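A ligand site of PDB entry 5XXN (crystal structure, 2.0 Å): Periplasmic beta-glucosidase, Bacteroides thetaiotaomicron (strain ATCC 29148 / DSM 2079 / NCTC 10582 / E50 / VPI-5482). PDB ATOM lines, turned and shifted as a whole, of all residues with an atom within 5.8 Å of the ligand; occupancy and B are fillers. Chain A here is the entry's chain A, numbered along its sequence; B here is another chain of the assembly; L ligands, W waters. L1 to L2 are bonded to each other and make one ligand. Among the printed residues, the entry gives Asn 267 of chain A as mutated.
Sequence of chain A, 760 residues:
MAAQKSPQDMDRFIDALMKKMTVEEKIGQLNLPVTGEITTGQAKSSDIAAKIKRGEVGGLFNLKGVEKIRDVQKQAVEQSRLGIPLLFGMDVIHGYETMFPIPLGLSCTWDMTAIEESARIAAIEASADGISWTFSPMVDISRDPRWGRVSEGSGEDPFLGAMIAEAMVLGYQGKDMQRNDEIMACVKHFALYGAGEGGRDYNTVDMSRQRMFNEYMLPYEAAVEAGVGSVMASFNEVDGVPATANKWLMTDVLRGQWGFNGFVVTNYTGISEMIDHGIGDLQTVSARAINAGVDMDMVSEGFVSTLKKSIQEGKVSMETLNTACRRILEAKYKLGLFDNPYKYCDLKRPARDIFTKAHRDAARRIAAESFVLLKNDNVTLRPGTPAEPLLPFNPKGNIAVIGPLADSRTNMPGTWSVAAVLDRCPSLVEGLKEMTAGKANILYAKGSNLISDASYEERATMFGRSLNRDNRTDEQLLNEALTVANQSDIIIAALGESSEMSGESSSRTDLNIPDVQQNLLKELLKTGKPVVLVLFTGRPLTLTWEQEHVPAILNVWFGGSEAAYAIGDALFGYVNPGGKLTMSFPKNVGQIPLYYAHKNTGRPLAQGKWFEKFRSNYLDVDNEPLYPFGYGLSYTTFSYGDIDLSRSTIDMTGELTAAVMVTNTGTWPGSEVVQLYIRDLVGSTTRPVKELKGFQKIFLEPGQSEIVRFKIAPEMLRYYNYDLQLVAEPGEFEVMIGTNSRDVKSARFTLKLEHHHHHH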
ATOM      1  N   PHE A  61      -1.014   0.504   3.945  1.00  0.00           N
ATOM      2  CA  PHE A  61      -1.582   1.065   2.729  1.00  0.00           C
ATOM      3  C   PHE A  61      -2.359   2.329   3.040  1.00  0.00           C
ATOM      4  O   PHE A  61      -2.667   2.622   4.210  1.00  0.00           O
ATOM      5  CB  PHE A  61      -2.441   0.021   1.981  1.00  0.00           C
ATOM      6  CG  PHE A  61      -3.717  -0.343   2.691  1.00  0.00           C
ATOM      7  CD1 PHE A  61      -3.694  -1.051   3.885  1.00  0.00           C
ATOM      8  CD2 PHE A  61      -4.956   0.010   2.152  1.00  0.00           C
ATOM      9  CE1 PHE A  61      -4.868  -1.377   4.532  1.00  0.00           C
ATOM     10  CE2 PHE A  61      -6.123  -0.320   2.803  1.00  0.00           C
ATOM     11  CZ  PHE A  61      -6.086  -1.017   3.989  1.00  0.00           C
ATOM     12  N   ASN A  62      -2.660   3.057   1.973  1.00  0.00           N
ATOM     13  CA  ASN A  62      -3.330   4.360   2.019  1.00  0.00           C
ATOM     14  C   ASN A  62      -2.531   5.493   2.642  1.00  0.00           C
ATOM     15  O   ASN A  62      -3.100   6.526   2.992  1.00  0.00           O
ATOM     16  CB  ASN A  62      -4.739   4.247   2.626  1.00  0.00           C
ATOM     17  CG  ASN A  62      -5.710   3.583   1.677  1.00  0.00           C
ATOM     18  OD1 ASN A  62      -5.375   3.288   0.526  1.00  0.00           O
ATOM     19  ND2 ASN A  62      -6.919   3.323   2.141  1.00  0.00           N
ATOM     20  N   ASP A  91      -4.519   2.103  -3.884  1.00  0.00           N
ATOM     21  CA  ASP A  91      -5.364   1.889  -5.059  1.00  0.00           C
ATOM     22  C   ASP A  91      -4.925   2.803  -6.199  1.00  0.00           C
ATOM     23  O   ASP A  91      -5.391   3.933  -6.325  1.00  0.00           O
ATOM     24  CB  ASP A  91      -6.809   2.092  -4.682  1.00  0.00           C
ATOM     25  CG  ASP A  91      -7.326   0.957  -3.824  1.00  0.00           C
ATOM     26  OD1 ASP A  91      -7.464  -0.151  -4.371  1.00  0.00           O
ATOM     27  OD2 ASP A  91      -7.589   1.162  -2.625  1.00  0.00           O
ATOM     28  N   PHE A 135      -3.202  -2.057  -5.793  1.00  0.00           N
ATOM     29  CA  PHE A 135      -4.339  -2.964  -5.739  1.00  0.00           C
ATOM     30  C   PHE A 135      -5.082  -2.871  -7.068  1.00  0.00           C
ATOM     31  O   PHE A 135      -6.241  -2.428  -7.142  1.00  0.00           O
ATOM     32  CB  PHE A 135      -5.234  -2.617  -4.533  1.00  0.00           C
ATOM     33  CG  PHE A 135      -4.517  -2.617  -3.195  1.00  0.00           C
ATOM     34  CD1 PHE A 135      -3.729  -3.693  -2.814  1.00  0.00           C
ATOM     35  CD2 PHE A 135      -4.645  -1.554  -2.328  1.00  0.00           C
ATOM     36  CE1 PHE A 135      -3.091  -3.701  -1.571  1.00  0.00           C
ATOM     37  CE2 PHE A 135      -4.007  -1.552  -1.095  1.00  0.00           C
ATOM     38  CZ  PHE A 135      -3.219  -2.628  -0.714  1.00  0.00           C
ATOM     39  N   ARG A 149     -19.310  -1.053  -9.515  1.00  0.00           N
ATOM     40  CA  ARG A 149     -17.924  -1.387  -9.742  1.00  0.00           C
ATOM     41  C   ARG A 149     -17.612  -1.849 -11.176  1.00  0.00           C
ATOM     42  O   ARG A 149     -16.458  -2.125 -11.479  1.00  0.00           O
ATOM     43  CB  ARG A 149     -17.422  -2.396  -8.712  1.00  0.00           C
ATOM     44  CG  ARG A 149     -17.765  -2.024  -7.282  1.00  0.00           C
ATOM     45  CD  ARG A 149     -16.881  -2.732  -6.251  1.00  0.00           C
ATOM     46  NE  ARG A 149     -15.524  -2.170  -6.256  1.00  0.00           N
ATOM     47  CZ  ARG A 149     -14.576  -2.419  -5.357  1.00  0.00           C
ATOM     48  NH1 ARG A 149     -14.792  -3.234  -4.348  1.00  0.00           N
ATOM     49  NH2 ARG A 149     -13.382  -1.844  -5.498  1.00  0.00           N
ATOM     50  N   GLU A 152     -14.745   0.041 -12.762  1.00  0.00           N
ATOM     51  CA  GLU A 152     -13.394  -0.367 -12.390  1.00  0.00           C
ATOM     52  C   GLU A 152     -12.820  -1.507 -13.181  1.00  0.00           C
ATOM     53  O   GLU A 152     -11.629  -1.781 -13.066  1.00  0.00           O
ATOM     54  CB  GLU A 152     -13.393  -0.831 -10.932  1.00  0.00           C
ATOM     55  CG  GLU A 152     -13.685   0.276  -9.974  1.00  0.00           C
ATOM     56  CD  GLU A 152     -13.911  -0.224  -8.589  1.00  0.00           C
ATOM     57  OE1 GLU A 152     -15.015   0.068  -8.066  1.00  0.00           O
ATOM     58  OE2 GLU A 152     -12.993  -0.878  -8.018  1.00  0.00           O
ATOM     59  N   LYS A 188      -7.583  -8.427  -8.654  1.00  0.00           N
ATOM     60  CA  LYS A 188      -8.739  -8.427  -7.758  1.00  0.00           C
ATOM     61  C   LYS A 188     -10.012  -8.456  -8.579  1.00  0.00           C
ATOM     62  O   LYS A 188      -9.970  -8.091  -9.744  1.00  0.00           O
ATOM     63  CB  LYS A 188      -8.722  -7.197  -6.850  1.00  0.00           C
ATOM     64  CG  LYS A 188      -9.059  -5.852  -7.489  1.00  0.00           C
ATOM     65  CD  LYS A 188      -8.568  -4.693  -6.614  1.00  0.00           C
ATOM     66  CE  LYS A 188      -9.094  -3.343  -7.090  1.00  0.00           C
ATOM     67  NZ  LYS A 188      -8.878  -2.271  -6.060  1.00  0.00           N
ATOM     68  N   HIS A 189     -11.140  -8.889  -8.021  1.00  0.00           N
ATOM     69  CA  HIS A 189     -11.292  -9.418  -6.668  1.00  0.00           C
ATOM     70  C   HIS A 189     -11.628 -10.924  -6.803  1.00  0.00           C
ATOM     71  O   HIS A 189     -12.699 -11.293  -7.314  1.00  0.00           O
ATOM     72  CB  HIS A 189     -12.398  -8.692  -5.902  1.00  0.00           C
ATOM     73  CG  HIS A 189     -12.260  -7.195  -5.874  1.00  0.00           C
ATOM     74  ND1 HIS A 189     -12.681  -6.391  -6.901  1.00  0.00           N
ATOM     75  CD2 HIS A 189     -11.802  -6.352  -4.910  1.00  0.00           C
ATOM     76  CE1 HIS A 189     -12.465  -5.114  -6.589  1.00  0.00           C
ATOM     77  NE2 HIS A 189     -11.919  -5.073  -5.387  1.00  0.00           N
ATOM     78  N   TYR A 193     -17.029 -11.662  -8.106  1.00  0.00           N
ATOM     79  CA  TYR A 193     -17.614 -10.538  -7.355  1.00  0.00           C
ATOM     80  C   TYR A 193     -18.572  -9.708  -8.207  1.00  0.00           C
ATOM     81  O   TYR A 193     -19.526  -9.150  -7.691  1.00  0.00           O
ATOM     82  CB  TYR A 193     -16.431  -9.715  -6.833  1.00  0.00           C
ATOM     83  CG  TYR A 193     -16.677  -8.453  -6.061  1.00  0.00           C
ATOM     84  CD1 TYR A 193     -17.690  -8.352  -5.145  1.00  0.00           C
ATOM     85  CD2 TYR A 193     -15.812  -7.370  -6.219  1.00  0.00           C
ATOM     86  CE1 TYR A 193     -17.878  -7.180  -4.422  1.00  0.00           C
ATOM     87  CE2 TYR A 193     -15.979  -6.202  -5.489  1.00  0.00           C
ATOM     88  CZ  TYR A 193     -17.019  -6.105  -4.600  1.00  0.00           C
ATOM     89  OH  TYR A 193     -17.214  -4.967  -3.860  1.00  0.00           O
ATOM     90  N   TYR A 202     -21.609  -6.333  -2.741  1.00  0.00           N
ATOM     91  CA  TYR A 202     -21.348  -7.265  -1.658  1.00  0.00           C
ATOM     92  C   TYR A 202     -22.349  -8.433  -1.534  1.00  0.00           C
ATOM     93  O   TYR A 202     -22.145  -9.319  -0.699  1.00  0.00           O
ATOM     94  CB  TYR A 202     -21.263  -6.524  -0.321  1.00  0.00           C
ATOM     95  CG  TYR A 202     -20.504  -5.197  -0.332  1.00  0.00           C
ATOM     96  CD1 TYR A 202     -19.181  -5.112  -0.790  1.00  0.00           C
ATOM     97  CD2 TYR A 202     -21.110  -4.034   0.154  1.00  0.00           C
ATOM     98  CE1 TYR A 202     -18.498  -3.894  -0.764  1.00  0.00           C
ATOM     99  CE2 TYR A 202     -20.426  -2.827   0.189  1.00  0.00           C
ATOM    100  CZ  TYR A 202     -19.130  -2.756  -0.286  1.00  0.00           C
ATOM    101  OH  TYR A 202     -18.470  -1.536  -0.225  1.00  0.00           O
ATOM    102  N   MET A 232      -6.034 -10.444  -4.553  1.00  0.00           N
ATOM    103  CA  MET A 232      -6.898 -10.009  -3.462  1.00  0.00           C
ATOM    104  C   MET A 232      -8.191 -10.820  -3.470  1.00  0.00           C
ATOM    105  O   MET A 232      -8.866 -10.922  -4.498  1.00  0.00           O
ATOM    106  CB  MET A 232      -7.201  -8.502  -3.544  1.00  0.00           C
ATOM    107  CG  MET A 232      -8.112  -7.973  -2.434  1.00  0.00           C
ATOM    108  SD  MET A 232      -8.494  -6.200  -2.600  1.00  0.00           S
ATOM    109  CE  MET A 232      -6.883  -5.501  -2.257  1.00  0.00           C
ATOM    110  N   PHE A 235     -15.172  -9.939  -1.564  1.00  0.00           N
ATOM    111  CA  PHE A 235     -16.121  -9.797  -0.463  1.00  0.00           C
ATOM    112  C   PHE A 235     -17.247 -10.840  -0.476  1.00  0.00           C
ATOM    113  O   PHE A 235     -17.875 -11.099   0.559  1.00  0.00           O
ATOM    114  CB  PHE A 235     -16.776  -8.419  -0.482  1.00  0.00           C
ATOM    115  CG  PHE A 235     -15.897  -7.299   0.000  1.00  0.00           C
ATOM    116  CD1 PHE A 235     -15.241  -7.372   1.234  1.00  0.00           C
ATOM    117  CD2 PHE A 235     -15.772  -6.133  -0.740  1.00  0.00           C
ATOM    118  CE1 PHE A 235     -14.449  -6.316   1.696  1.00  0.00           C
ATOM    119  CE2 PHE A 235     -14.987  -5.078  -0.291  1.00  0.00           C
ATOM    120  CZ  PHE A 235     -14.329  -5.164   0.928  1.00  0.00           C
ATOM    121  N   ASN A 267      -9.500  -8.440   1.132  1.00  0.00           N
ATOM    122  CA  ASN A 267      -9.992  -7.095   0.918  1.00  0.00           C
ATOM    123  C   ASN A 267     -10.174  -6.514   2.328  1.00  0.00           C
ATOM    124  O   ASN A 267      -9.927  -7.189   3.329  1.00  0.00           O
ATOM    125  CB  ASN A 267     -11.304  -7.073   0.101  1.00  0.00           C
ATOM    126  CG  ASN A 267     -11.502  -5.761  -0.681  1.00  0.00           C
ATOM    127  OD1 ASN A 267     -11.005  -4.712  -0.272  1.00  0.00           O
ATOM    128  ND2 ASN A 267     -12.216  -5.829  -1.797  1.00  0.00           N
ATOM    129  N   TYR A 268     -10.601  -5.247   2.379  1.00  0.00           N
ATOM    130  CA  TYR A 268     -10.737  -4.477   3.599  1.00  0.00           C
ATOM    131  C   TYR A 268     -11.698  -5.072   4.668  1.00  0.00           C
ATOM    132  O   TYR A 268     -12.895  -5.132   4.473  1.00  0.00           O
ATOM    133  CB  TYR A 268     -11.193  -3.056   3.215  1.00  0.00           C
ATOM    134  CG  TYR A 268     -10.934  -1.978   4.230  1.00  0.00           C
ATOM    135  CD1 TYR A 268     -11.715  -1.870   5.379  1.00  0.00           C
ATOM    136  CD2 TYR A 268      -9.946  -1.035   4.022  1.00  0.00           C
ATOM    137  CE1 TYR A 268     -11.524  -0.849   6.277  1.00  0.00           C
ATOM    138  CE2 TYR A 268      -9.734  -0.001   4.924  1.00  0.00           C
ATOM    139  CZ  TYR A 268     -10.512   0.087   6.051  1.00  0.00           C
ATOM    140  OH  TYR A 268     -10.299   1.097   6.947  1.00  0.00           O
ATOM    141  N   GLU A 273     -15.432  -9.613   8.447  1.00  0.00           N
ATOM    142  CA  GLU A 273     -16.705  -9.647   7.738  1.00  0.00           C
ATOM    143  C   GLU A 273     -17.293 -11.060   7.588  1.00  0.00           C
ATOM    144  O   GLU A 273     -18.496 -11.210   7.431  1.00  0.00           O
ATOM    145  CB  GLU A 273     -16.562  -8.943   6.390  1.00  0.00           C
ATOM    146  CG  GLU A 273     -16.577  -7.427   6.586  1.00  0.00           C
ATOM    147  CD  GLU A 273     -16.127  -6.644   5.363  1.00  0.00           C
ATOM    148  OE1 GLU A 273     -16.249  -7.145   4.211  1.00  0.00           O
ATOM    149  OE2 GLU A 273     -15.663  -5.504   5.554  1.00  0.00           O
ATOM    150  N   MET A 298      -5.802  -7.670   5.644  1.00  0.00           N
ATOM    151  CA  MET A 298      -6.114  -6.234   5.545  1.00  0.00           C
ATOM    152  C   MET A 298      -7.073  -5.727   6.642  1.00  0.00           C
ATOM    153  O   MET A 298      -8.293  -5.991   6.611  1.00  0.00           O
ATOM    154  CB  MET A 298      -6.658  -5.908   4.150  1.00  0.00           C
ATOM    155  CG  MET A 298      -6.618  -4.420   3.814  1.00  0.00           C
ATOM    156  SD  MET A 298      -7.393  -4.065   2.236  1.00  0.00           S
ATOM    157  CE  MET A 298      -5.987  -3.995   1.143  1.00  0.00           C
ATOM    158  N   TRP A 416     -12.359   6.276  -7.874  1.00  0.00           N
ATOM    159  CA  TRP A 416     -11.063   5.604  -7.663  1.00  0.00           C
ATOM    160  C   TRP A 416      -9.895   6.424  -8.252  1.00  0.00           C
ATOM    161  O   TRP A 416      -9.109   5.945  -9.085  1.00  0.00           O
ATOM    162  CB  TRP A 416     -11.108   4.155  -8.178  1.00  0.00           C
ATOM    163  CG  TRP A 416     -11.862   3.279  -7.254  1.00  0.00           C
ATOM    164  CD1 TRP A 416     -13.094   2.684  -7.487  1.00  0.00           C
ATOM    165  CD2 TRP A 416     -11.488   2.920  -5.929  1.00  0.00           C
ATOM    166  NE1 TRP A 416     -13.476   1.954  -6.384  1.00  0.00           N
ATOM    167  CE2 TRP A 416     -12.509   2.092  -5.411  1.00  0.00           C
ATOM    168  CE3 TRP A 416     -10.353   3.196  -5.128  1.00  0.00           C
ATOM    169  CZ2 TRP A 416     -12.435   1.530  -4.126  1.00  0.00           C
ATOM    170  CZ3 TRP A 416     -10.294   2.651  -3.846  1.00  0.00           C
ATOM    171  CH2 TRP A 416     -11.336   1.831  -3.351  1.00  0.00           C
ATOM    172  N   GLU A 504     -17.334   1.712  -5.656  1.00  0.00           N
ATOM    173  CA  GLU A 504     -17.714   0.758  -4.635  1.00  0.00           C
ATOM    174  C   GLU A 504     -18.902   1.299  -3.874  1.00  0.00           C
ATOM    175  O   GLU A 504     -18.993   2.496  -3.591  1.00  0.00           O
ATOM    176  CB  GLU A 504     -16.539   0.471  -3.691  1.00  0.00           C
ATOM    177  CG  GLU A 504     -16.927  -0.390  -2.513  1.00  0.00           C
ATOM    178  CD  GLU A 504     -15.749  -0.970  -1.739  1.00  0.00           C
ATOM    179  OE1 GLU A 504     -14.595  -0.806  -2.163  1.00  0.00           O
ATOM    180  OE2 GLU A 504     -16.004  -1.602  -0.695  1.00  0.00           O
ATOM    181  N   ARG B 603     -21.497  -7.653   4.692  1.00  0.00           N
ATOM    182  CA  ARG B 603     -21.743  -6.253   5.033  1.00  0.00           C
ATOM    183  C   ARG B 603     -23.231  -5.909   5.078  1.00  0.00           C
ATOM    184  O   ARG B 603     -23.691  -5.068   4.296  1.00  0.00           O
ATOM    185  CB  ARG B 603     -21.028  -5.353   4.029  1.00  0.00           C
ATOM    186  CG  ARG B 603     -19.528  -5.537   4.004  1.00  0.00           C
ATOM    187  CD  ARG B 603     -18.874  -4.596   3.024  1.00  0.00           C
ATOM    188  NE  ARG B 603     -17.441  -4.533   3.309  1.00  0.00           N
ATOM    189  CZ  ARG B 603     -16.631  -3.494   3.049  1.00  0.00           C
ATOM    190  NH1 ARG B 603     -17.066  -2.380   2.458  1.00  0.00           N
ATOM    191  NH2 ARG B 603     -15.350  -3.581   3.398  1.00  0.00           N
ATOM    192  N   PHE B 614     -20.614   1.873   1.993  1.00  0.00           N
ATOM    193  CA  PHE B 614     -19.894   0.622   2.335  1.00  0.00           C
ATOM    194  C   PHE B 614     -20.651  -0.503   3.064  1.00  0.00           C
ATOM    195  O   PHE B 614     -20.022  -1.440   3.601  1.00  0.00           O
ATOM    196  CB  PHE B 614     -18.586   0.944   3.061  1.00  0.00           C
ATOM    197  CG  PHE B 614     -17.728   1.914   2.318  1.00  0.00           C
ATOM    198  CD1 PHE B 614     -17.356   1.649   1.010  1.00  0.00           C
ATOM    199  CD2 PHE B 614     -17.278   3.110   2.914  1.00  0.00           C
ATOM    200  CE1 PHE B 614     -16.574   2.544   0.299  1.00  0.00           C
ATOM    201  CE2 PHE B 614     -16.475   3.994   2.202  1.00  0.00           C
ATOM    202  CZ  PHE B 614     -16.129   3.704   0.886  1.00  0.00           C
HETATM  203  C1  LIG L   1     -12.553  -0.075   1.108  1.00  0.00           C
HETATM  204  C2  LIG L   1     -13.987  -0.406   1.597  1.00  0.00           C
HETATM  205  C3  LIG L   1     -14.108   0.043   3.051  1.00  0.00           C
HETATM  206  C4  LIG L   1     -13.651   1.500   3.228  1.00  0.00           C
HETATM  207  C5  LIG L   1     -13.794   1.953   4.675  1.00  0.00           C
HETATM  208  C6  LIG L   1     -12.127   1.375   1.436  1.00  0.00           C
HETATM  209  O1  LIG L   1     -10.751   1.533   1.093  1.00  0.00           O
HETATM  210  O2  LIG L   1     -12.330  -0.362  -0.290  1.00  0.00           O
HETATM  211  O3  LIG L   1     -14.275  -1.796   1.392  1.00  0.00           O
HETATM  212  O4  LIG L   1     -15.471  -0.016   3.453  1.00  0.00           O
HETATM  213  O5  LIG L   1     -12.284   1.612   2.832  1.00  0.00           O
HETATM  214  O6  LIG L   1     -13.334   3.298   4.778  1.00  0.00           O
HETATM  215  C1  LG2 L   2     -11.782  -1.907  -2.039  1.00  0.00           C
HETATM  216  C2  LG2 L   2     -10.581  -2.554  -2.705  1.00  0.00           C
HETATM  217  C3  LG2 L   2      -9.331  -1.782  -2.304  1.00  0.00           C
HETATM  218  C4  LG2 L   2      -9.193  -1.911  -0.807  1.00  0.00           C
HETATM  219  C5  LG2 L   2      -7.887  -1.351  -0.239  1.00  0.00           C
HETATM  220  C6  LG2 L   2     -11.575  -1.546  -0.553  1.00  0.00           C
HETATM  221  O1  LG2 L   2     -12.836  -2.837  -2.158  1.00  0.00           O
HETATM  222  O2  LG2 L   2     -10.741  -2.676  -4.102  1.00  0.00           O
HETATM  223  O3  LG2 L   2      -8.241  -2.393  -2.920  1.00  0.00           O
HETATM  224  O4  LG2 L   2     -10.252  -1.211  -0.186  1.00  0.00           O
HETATM  225  O5  LG2 L   2      -7.831   0.066  -0.431  1.00  0.00           O
HETATM  226  O   HOH W   1     -13.768   1.731  -1.161  1.00  0.00           O
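Merely in contact with the ligand: Phe 614 of chain B (3.2 Å), Phe 235 (3.4 Å), Phe 135 (3.4 Å), Met 232 (3.5 Å), Met 298 (3.5 Å), Phe 61 (3.7 Å), Tyr 268 (3.7 Å) and Trp 416 (3.9 Å). Within 4 Å of the ligand: Phe 61, Asp 91, Phe 135, Arg 149, Lys 188, His 189, Met 232, Phe 235, Asn 267, Tyr 268, Met 298, Trp 416, Glu 504, Arg 603 of chain B and Phe 614 of chain B. The nearest printed residue that does not touch the ligand is Asn 62 (4.2 Å).
Water W1 lies within hydrogen-bond range of O2 of LIG L1 (2.7 Å) and OE1 of Glu 504 (2.9 Å).
The backbone carbonyl oxygen (O) of Phe 135 is in hydrogen-bond range of the side-chain amino group (NZ) of Lys 188 (2.9 Å). SD of Met 232 sits close to OD1 of Asn 267 (3.7 Å). The indole nitrogen of Trp 416 lies within hydrogen-bond range of the side-chain carboxylate of Glu 152 (3.0 Å). The guanidinium group of Arg 149 lies within salt-bridge range of the side-chain carboxylate of Glu 504 (3.3 Å). The guanidinium group (NH2) of Arg 603 of chain B lies within hydrogen-bond range of the backbone carbonyl oxygen (O) of Tyr 268, 3.1 Å away. OE2 of Glu 504 lies within salt-bridge range of NH1 of Arg 603 of chain B, at 3.4 Å. SD of Met 298 is in hydrogen-bond range of N of Tyr 268 (3.4 Å). The backbone carbonyl oxygen of Phe 614 of chain B sits at hydrogen-bond distance from the guanidinium group of Arg 603 of chain B (3.3 Å).
NH1 of Arg 149 sits at hydrogen-bond distance from O1 of LG2 L2, at 3.0 Å. A ring nitrogen (NE2) of His 189 lies within hydrogen-bond range of an oxygen (O2) of LG2 L2 (3.0 Å). O3 of LIG L1 is in hydrogen-bond range of NH2 of Arg 603 of chain B (2.9 Å). The side-chain carboxylate (OD2) of Asp 91 lies within hydrogen-bond range of an oxygen (O5) of LG2 L2 (2.5 Å). ND2 of Asn 267 is in hydrogen-bond range of O1 of LG2 L2, 3.1 Å away. An oxygen (O2) of LG2 L2 lies within hydrogen-bond range of the side-chain amino group of Lys 188. The side-chain carboxylate (OE1) of Glu 504 sits at hydrogen-bond distance from an oxygen (O1) of LG2 L2 (2.7 Å).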
